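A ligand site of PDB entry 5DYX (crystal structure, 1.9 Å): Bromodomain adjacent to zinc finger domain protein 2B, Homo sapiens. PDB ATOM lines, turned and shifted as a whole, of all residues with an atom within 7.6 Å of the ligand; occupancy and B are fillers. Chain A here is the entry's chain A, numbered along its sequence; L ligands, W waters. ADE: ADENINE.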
ATOM      1  N   TRP A  32     -24.413 -16.711  18.234  1.00  0.00           N
ATOM      2  CA  TRP A  32     -24.451 -16.738  19.699  1.00  0.00           C
ATOM      3  C   TRP A  32     -24.335 -18.118  20.369  1.00  0.00           C
ATOM      4  O   TRP A  32     -23.766 -18.205  21.464  1.00  0.00           O
ATOM      5  CB  TRP A  32     -25.723 -16.041  20.216  1.00  0.00           C
ATOM      6  CG  TRP A  32     -27.003 -16.576  19.668  1.00  0.00           C
ATOM      7  CD1 TRP A  32     -27.646 -16.155  18.530  1.00  0.00           C
ATOM      8  CD2 TRP A  32     -27.826 -17.604  20.242  1.00  0.00           C
ATOM      9  NE1 TRP A  32     -28.802 -16.872  18.360  1.00  0.00           N
ATOM     10  CE2 TRP A  32     -28.938 -17.765  19.386  1.00  0.00           C
ATOM     11  CE3 TRP A  32     -27.714 -18.417  21.375  1.00  0.00           C
ATOM     12  CZ2 TRP A  32     -29.941 -18.717  19.637  1.00  0.00           C
ATOM     13  CZ3 TRP A  32     -28.701 -19.356  21.619  1.00  0.00           C
ATOM     14  CH2 TRP A  32     -29.807 -19.495  20.759  1.00  0.00           C
ATOM     15  N   PRO A  33     -24.861 -19.198  19.749  1.00  0.00           N
ATOM     16  CA  PRO A  33     -24.679 -20.470  20.461  1.00  0.00           C
ATOM     17  C   PRO A  33     -23.241 -21.002  20.419  1.00  0.00           C
ATOM     18  O   PRO A  33     -22.934 -21.990  21.105  1.00  0.00           O
ATOM     19  CB  PRO A  33     -25.598 -21.450  19.710  1.00  0.00           C
ATOM     20  CG  PRO A  33     -26.504 -20.587  18.846  1.00  0.00           C
ATOM     21  CD  PRO A  33     -25.659 -19.402  18.523  1.00  0.00           C
ATOM     22  N   PHE A  34     -22.382 -20.356  19.639  1.00  0.00           N
ATOM     23  CA  PHE A  34     -21.069 -20.907  19.284  1.00  0.00           C
ATOM     24  C   PHE A  34     -19.912 -20.009  19.665  1.00  0.00           C
ATOM     25  O   PHE A  34     -18.772 -20.339  19.353  1.00  0.00           O
ATOM     26  CB  PHE A  34     -21.014 -21.184  17.768  1.00  0.00           C
ATOM     27  CG  PHE A  34     -22.234 -21.901  17.248  1.00  0.00           C
ATOM     28  CD1 PHE A  34     -22.526 -23.189  17.694  1.00  0.00           C
ATOM     29  CD2 PHE A  34     -23.097 -21.282  16.374  1.00  0.00           C
ATOM     30  CE1 PHE A  34     -23.666 -23.857  17.242  1.00  0.00           C
ATOM     31  CE2 PHE A  34     -24.241 -21.942  15.912  1.00  0.00           C
ATOM     32  CZ  PHE A  34     -24.521 -23.223  16.340  1.00  0.00           C
ATOM     33  N   LEU A  35     -20.181 -18.890  20.310  1.00  0.00           N
ATOM     34  CA  LEU A  35     -19.127 -17.903  20.586  1.00  0.00           C
ATOM     35  C   LEU A  35     -18.203 -18.380  21.683  1.00  0.00           C
ATOM     36  O   LEU A  35     -17.005 -18.103  21.649  1.00  0.00           O
ATOM     37  CB  LEU A  35     -19.741 -16.551  20.964  1.00  0.00           C
ATOM     38  CG  LEU A  35     -20.553 -15.887  19.847  1.00  0.00           C
ATOM     39  CD1 LEU A  35     -21.210 -14.617  20.357  1.00  0.00           C
ATOM     40  CD2 LEU A  35     -19.646 -15.578  18.642  1.00  0.00           C
ATOM     41  N   LEU A  36     -18.753 -19.097  22.658  1.00  0.00           N
ATOM     42  CA  LEU A  36     -17.998 -19.582  23.817  1.00  0.00           C
ATOM     43  C   LEU A  36     -18.193 -21.075  24.004  1.00  0.00           C
ATOM     44  O   LEU A  36     -19.161 -21.631  23.503  1.00  0.00           O
ATOM     45  CB  LEU A  36     -18.453 -18.835  25.076  1.00  0.00           C
ATOM     46  CG  LEU A  36     -18.250 -17.335  25.045  1.00  0.00           C
ATOM     47  CD1 LEU A  36     -18.792 -16.713  26.332  1.00  0.00           C
ATOM     48  CD2 LEU A  36     -16.774 -17.019  24.877  1.00  0.00           C
ATOM     49  N   PRO A  37     -17.279 -21.740  24.734  1.00  0.00           N
ATOM     50  CA  PRO A  37     -17.483 -23.166  24.983  1.00  0.00           C
ATOM     51  C   PRO A  37     -18.816 -23.425  25.685  1.00  0.00           C
ATOM     52  O   PRO A  37     -19.245 -22.609  26.502  1.00  0.00           O
ATOM     53  CB  PRO A  37     -16.309 -23.551  25.905  1.00  0.00           C
ATOM     54  CG  PRO A  37     -15.279 -22.542  25.622  1.00  0.00           C
ATOM     55  CD  PRO A  37     -15.986 -21.263  25.272  1.00  0.00           C
ATOM     56  N   VAL A  38     -19.467 -24.525  25.337  1.00  0.00           N
ATOM     57  CA  VAL A  38     -20.636 -24.966  26.091  1.00  0.00           C
ATOM     58  C   VAL A  38     -20.209 -25.224  27.521  1.00  0.00           C
ATOM     59  O   VAL A  38     -19.150 -25.825  27.766  1.00  0.00           O
ATOM     60  CB  VAL A  38     -21.262 -26.239  25.473  1.00  0.00           C
ATOM     61  CG1 VAL A  38     -22.424 -26.736  26.339  1.00  0.00           C
ATOM     62  CG2 VAL A  38     -21.728 -25.964  24.051  1.00  0.00           C
ATOM     63  N   ASN A  39     -21.003 -24.733  28.472  1.00  0.00           N
ATOM     64  CA  ASN A  39     -20.681 -24.879  29.895  1.00  0.00           C
ATOM     65  C   ASN A  39     -20.946 -26.297  30.374  1.00  0.00           C
ATOM     66  O   ASN A  39     -22.094 -26.679  30.597  1.00  0.00           O
ATOM     67  CB  ASN A  39     -21.492 -23.870  30.724  1.00  0.00           C
ATOM     68  CG  ASN A  39     -20.986 -23.750  32.157  1.00  0.00           C
ATOM     69  OD1 ASN A  39     -20.511 -24.716  32.749  1.00  0.00           O
ATOM     70  ND2 ASN A  39     -21.113 -22.557  32.717  1.00  0.00           N
ATOM     71  N   LEU A  42     -23.203 -26.728  33.418  1.00  0.00           N
ATOM     72  CA  LEU A  42     -24.568 -26.248  33.413  1.00  0.00           C
ATOM     73  C   LEU A  42     -25.414 -26.948  32.360  1.00  0.00           C
ATOM     74  O   LEU A  42     -26.630 -26.766  32.321  1.00  0.00           O
ATOM     75  CB  LEU A  42     -24.615 -24.732  33.199  1.00  0.00           C
ATOM     76  CG  LEU A  42     -23.821 -23.855  34.170  1.00  0.00           C
ATOM     77  CD1 LEU A  42     -24.196 -22.391  33.999  1.00  0.00           C
ATOM     78  CD2 LEU A  42     -24.036 -24.302  35.611  1.00  0.00           C
ATOM     79  N   VAL A  43     -24.785 -27.724  31.495  1.00  0.00           N
ATOM     80  CA  VAL A  43     -25.523 -28.386  30.428  1.00  0.00           C
ATOM     81  C   VAL A  43     -25.413 -29.890  30.582  1.00  0.00           C
ATOM     82  O   VAL A  43     -24.389 -30.480  30.227  1.00  0.00           O
ATOM     83  CB  VAL A  43     -25.040 -27.950  29.031  1.00  0.00           C
ATOM     84  CG1 VAL A  43     -25.886 -28.620  27.945  1.00  0.00           C
ATOM     85  CG2 VAL A  43     -25.100 -26.436  28.892  1.00  0.00           C
ATOM     86  N   PRO A  44     -26.481 -30.511  31.113  1.00  0.00           N
ATOM     87  CA  PRO A  44     -26.512 -31.948  31.388  1.00  0.00           C
ATOM     88  C   PRO A  44     -26.352 -32.739  30.100  1.00  0.00           C
ATOM     89  O   PRO A  44     -26.994 -32.439  29.094  1.00  0.00           O
ATOM     90  CB  PRO A  44     -27.910 -32.177  31.991  1.00  0.00           C
ATOM     91  CG  PRO A  44     -28.426 -30.816  32.347  1.00  0.00           C
ATOM     92  CD  PRO A  44     -27.782 -29.878  31.368  1.00  0.00           C
ATOM     93  N   TYR A  46     -23.826 -32.950  28.098  1.00  0.00           N
ATOM     94  CA  TYR A  46     -22.928 -32.456  27.047  1.00  0.00           C
ATOM     95  C   TYR A  46     -21.540 -33.089  27.107  1.00  0.00           C
ATOM     96  O   TYR A  46     -21.018 -33.531  26.085  1.00  0.00           O
ATOM     97  CB  TYR A  46     -22.793 -30.927  27.091  1.00  0.00           C
ATOM     98  CG  TYR A  46     -22.413 -30.394  25.721  1.00  0.00           C
ATOM     99  CD1 TYR A  46     -21.088 -30.181  25.382  1.00  0.00           C
ATOM    100  CD2 TYR A  46     -23.394 -30.175  24.752  1.00  0.00           C
ATOM    101  CE1 TYR A  46     -20.740 -29.707  24.109  1.00  0.00           C
ATOM    102  CE2 TYR A  46     -23.050 -29.708  23.485  1.00  0.00           C
ATOM    103  CZ  TYR A  46     -21.723 -29.483  23.181  1.00  0.00           C
ATOM    104  OH  TYR A  46     -21.359 -29.025  21.918  1.00  0.00           O
ATOM    105  N   ILE A  50     -20.641 -35.353  23.853  1.00  0.00           N
ATOM    106  CA  ILE A  50     -19.835 -34.644  22.848  1.00  0.00           C
ATOM    107  C   ILE A  50     -18.358 -34.811  23.152  1.00  0.00           C
ATOM    108  O   ILE A  50     -17.818 -34.142  24.028  1.00  0.00           O
ATOM    109  CB  ILE A  50     -20.185 -33.145  22.792  1.00  0.00           C
ATOM    110  CG1 ILE A  50     -21.672 -32.975  22.448  1.00  0.00           C
ATOM    111  CG2 ILE A  50     -19.258 -32.408  21.805  1.00  0.00           C
ATOM    112  CD1 ILE A  50     -22.065 -33.582  21.122  1.00  0.00           C
ATOM    113  N   MET A  54     -16.051 -27.884  20.627  1.00  0.00           N
ATOM    114  CA  MET A  54     -15.338 -26.849  19.892  1.00  0.00           C
ATOM    115  C   MET A  54     -16.267 -25.652  19.769  1.00  0.00           C
ATOM    116  O   MET A  54     -17.491 -25.798  19.771  1.00  0.00           O
ATOM    117  CB  MET A  54     -14.893 -27.377  18.528  1.00  0.00           C
ATOM    118  CG  MET A  54     -14.012 -26.412  17.723  1.00  0.00           C
ATOM    119  SD  MET A  54     -12.550 -25.857  18.662  1.00  0.00           S
ATOM    120  CE  MET A  54     -11.857 -27.433  19.142  1.00  0.00           C
ATOM    121  N   VAL A  81     -17.702 -27.781  15.141  1.00  0.00           N
ATOM    122  CA  VAL A  81     -18.673 -26.948  15.841  1.00  0.00           C
ATOM    123  C   VAL A  81     -20.107 -27.265  15.399  1.00  0.00           C
ATOM    124  O   VAL A  81     -21.012 -27.457  16.222  1.00  0.00           O
ATOM    125  CB  VAL A  81     -18.398 -25.442  15.604  1.00  0.00           C
ATOM    126  CG1 VAL A  81     -19.530 -24.594  16.185  1.00  0.00           C
ATOM    127  CG2 VAL A  81     -17.041 -25.042  16.198  1.00  0.00           C
ATOM    128  N   ASN A  84     -21.124 -31.064  16.163  1.00  0.00           N
ATOM    129  CA  ASN A  84     -21.498 -31.181  17.565  1.00  0.00           C
ATOM    130  C   ASN A  84     -22.904 -30.639  17.803  1.00  0.00           C
ATOM    131  O   ASN A  84     -23.691 -31.244  18.529  1.00  0.00           O
ATOM    132  CB  ASN A  84     -20.531 -30.432  18.470  1.00  0.00           C
ATOM    133  CG  ASN A  84     -19.192 -31.120  18.581  1.00  0.00           C
ATOM    134  OD1 ASN A  84     -19.041 -32.290  18.229  1.00  0.00           O
ATOM    135  ND2 ASN A  84     -18.202 -30.389  19.089  1.00  0.00           N
ATOM    136  N   CYS A  85     -23.197 -29.487  17.212  1.00  0.00           N
ATOM    137  CA  CYS A  85     -24.493 -28.836  17.386  1.00  0.00           C
ATOM    138  C   CYS A  85     -25.624 -29.729  16.888  1.00  0.00           C
ATOM    139  O   CYS A  85     -26.653 -29.870  17.557  1.00  0.00           O
ATOM    140  CB  CYS A  85     -24.520 -27.494  16.664  1.00  0.00           C
ATOM    141  SG  CYS A  85     -26.113 -26.587  16.762  1.00  0.00           S
ATOM    142  N   GLU A  86     -25.419 -30.352  15.722  1.00  0.00           N
ATOM    143  CA  GLU A  86     -26.403 -31.287  15.174  1.00  0.00           C
ATOM    144  C   GLU A  86     -26.607 -32.509  16.053  1.00  0.00           C
ATOM    145  O   GLU A  86     -27.720 -33.029  16.163  1.00  0.00           O
ATOM    146  CB  GLU A  86     -25.984 -31.748  13.786  1.00  0.00           C
ATOM    147  CG  GLU A  86     -26.483 -30.856  12.676  1.00  0.00           C
ATOM    148  CD  GLU A  86     -26.489 -31.571  11.343  1.00  0.00           C
ATOM    149  OE1 GLU A  86     -25.812 -31.105  10.412  1.00  0.00           O
ATOM    150  OE2 GLU A  86     -27.194 -32.600  11.221  1.00  0.00           O
ATOM    151  N   PHE A  88     -26.324 -32.677  19.300  1.00  0.00           N
ATOM    152  CA  PHE A  88     -26.963 -32.381  20.581  1.00  0.00           C
ATOM    153  C   PHE A  88     -28.298 -31.651  20.489  1.00  0.00           C
ATOM    154  O   PHE A  88     -29.055 -31.625  21.467  1.00  0.00           O
ATOM    155  CB  PHE A  88     -26.006 -31.552  21.438  1.00  0.00           C
ATOM    156  CG  PHE A  88     -26.243 -31.716  22.917  1.00  0.00           C
ATOM    157  CD1 PHE A  88     -25.785 -32.847  23.588  1.00  0.00           C
ATOM    158  CD2 PHE A  88     -26.918 -30.745  23.638  1.00  0.00           C
ATOM    159  CE1 PHE A  88     -25.996 -33.007  24.951  1.00  0.00           C
ATOM    160  CE2 PHE A  88     -27.133 -30.898  25.007  1.00  0.00           C
ATOM    161  CZ  PHE A  88     -26.675 -32.029  25.661  1.00  0.00           C
ATOM    162  N   ASN A  89     -28.608 -31.059  19.337  1.00  0.00           N
ATOM    163  CA  ASN A  89     -29.782 -30.209  19.215  1.00  0.00           C
ATOM    164  C   ASN A  89     -30.722 -30.645  18.105  1.00  0.00           C
ATOM    165  O   ASN A  89     -30.278 -31.030  17.027  1.00  0.00           O
ATOM    166  CB  ASN A  89     -29.359 -28.747  18.962  1.00  0.00           C
ATOM    167  CG  ASN A  89     -28.556 -28.163  20.103  1.00  0.00           C
ATOM    168  OD1 ASN A  89     -29.104 -27.624  21.068  1.00  0.00           O
ATOM    169  ND2 ASN A  89     -27.220 -28.245  19.985  1.00  0.00           N
ATOM    170  N   ILE A  95     -31.232 -23.233  18.438  1.00  0.00           N
ATOM    171  CA  ILE A  95     -29.809 -23.534  18.339  1.00  0.00           C
ATOM    172  C   ILE A  95     -29.557 -24.441  17.134  1.00  0.00           C
ATOM    173  O   ILE A  95     -28.612 -24.248  16.378  1.00  0.00           O
ATOM    174  CB  ILE A  95     -29.269 -24.197  19.644  1.00  0.00           C
ATOM    175  CG1 ILE A  95     -29.232 -23.162  20.766  1.00  0.00           C
ATOM    176  CG2 ILE A  95     -27.873 -24.781  19.433  1.00  0.00           C
ATOM    177  CD1 ILE A  95     -28.771 -23.715  22.098  1.00  0.00           C
ATOM    178  N   GLY A  96     -30.430 -25.437  16.964  1.00  0.00           N
ATOM    179  CA  GLY A  96     -30.366 -26.314  15.816  1.00  0.00           C
ATOM    180  C   GLY A  96     -30.410 -25.566  14.491  1.00  0.00           C
ATOM    181  O   GLY A  96     -29.604 -25.812  13.592  1.00  0.00           O
HETATM  182  N9  ADE L   1     -24.789 -26.157  21.151  1.00  0.00           N
HETATM  183  C8  ADE L   1     -24.296 -24.905  21.058  1.00  0.00           C
HETATM  184  N7  ADE L   1     -24.593 -24.227  22.208  1.00  0.00           N
HETATM  185  C5  ADE L   1     -25.298 -25.083  23.033  1.00  0.00           C
HETATM  186  C6  ADE L   1     -25.876 -24.971  24.359  1.00  0.00           C
HETATM  187  N6  ADE L   1     -25.795 -23.756  25.100  1.00  0.00           N
HETATM  188  N1  ADE L   1     -26.512 -26.043  24.874  1.00  0.00           N
HETATM  189  C2  ADE L   1     -26.605 -27.182  24.200  1.00  0.00           C
HETATM  190  N3  ADE L   1     -26.080 -27.325  22.991  1.00  0.00           N
HETATM  191  C4  ADE L   1     -25.419 -26.292  22.374  1.00  0.00           C
HETATM  192  O   HOH W   1     -23.134 -28.153  20.328  1.00  0.00           O
HETATM  193  O   HOH W   2     -24.114 -22.142  24.097  1.00  0.00           O
HETATM  194  O   HOH W   3     -28.698 -25.651  26.081  1.00  0.00           O
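The backbone carbonyl oxygen (O) of Cys 85 is in hydrogen-bond range of the side-chain amide nitrogen (ND2) of Asn 89 (3.0 Å). The side-chain sulfur (SG) of Cys 85 lies within hydrogen-bond range of the backbone carbonyl oxygen (O) of Ile 95, at 3.4 Å.
The backbone carbonyl oxygen (O) of Pro 33 sits close to a nitrogen (N7) of the ligand. ND2 of Asn 89 is in hydrogen-bond range of N3 of the ligand (3.3 Å).
Val 38 touches the ligand (CG2 to C5, 3.8 Å). CE2 of Tyr 46 touches N3 of the ligand, 3.9 Å away. CD2 of Phe 88 touches N3 of the ligand (3.6 Å). Ile 95 touches the ligand. Hydrophobic or aromatic side chains that line the ligand: Pro 33, Val 38, Tyr 46, Phe 88 and Ile 95. Six residues have an atom within 4 Å of the ligand: Pro 33, Val 38, Tyr 46, Phe 88, Asn 89 and Ile 95.
Water W2 lies within hydrogen-bond range of N6 of the ligand and O of Pro 33. Water W1 lies within hydrogen-bond range of OH of Tyr 46 (2.5 Å), N9 of the ligand (2.7 Å) and N of Cys 85 (3.4 Å).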
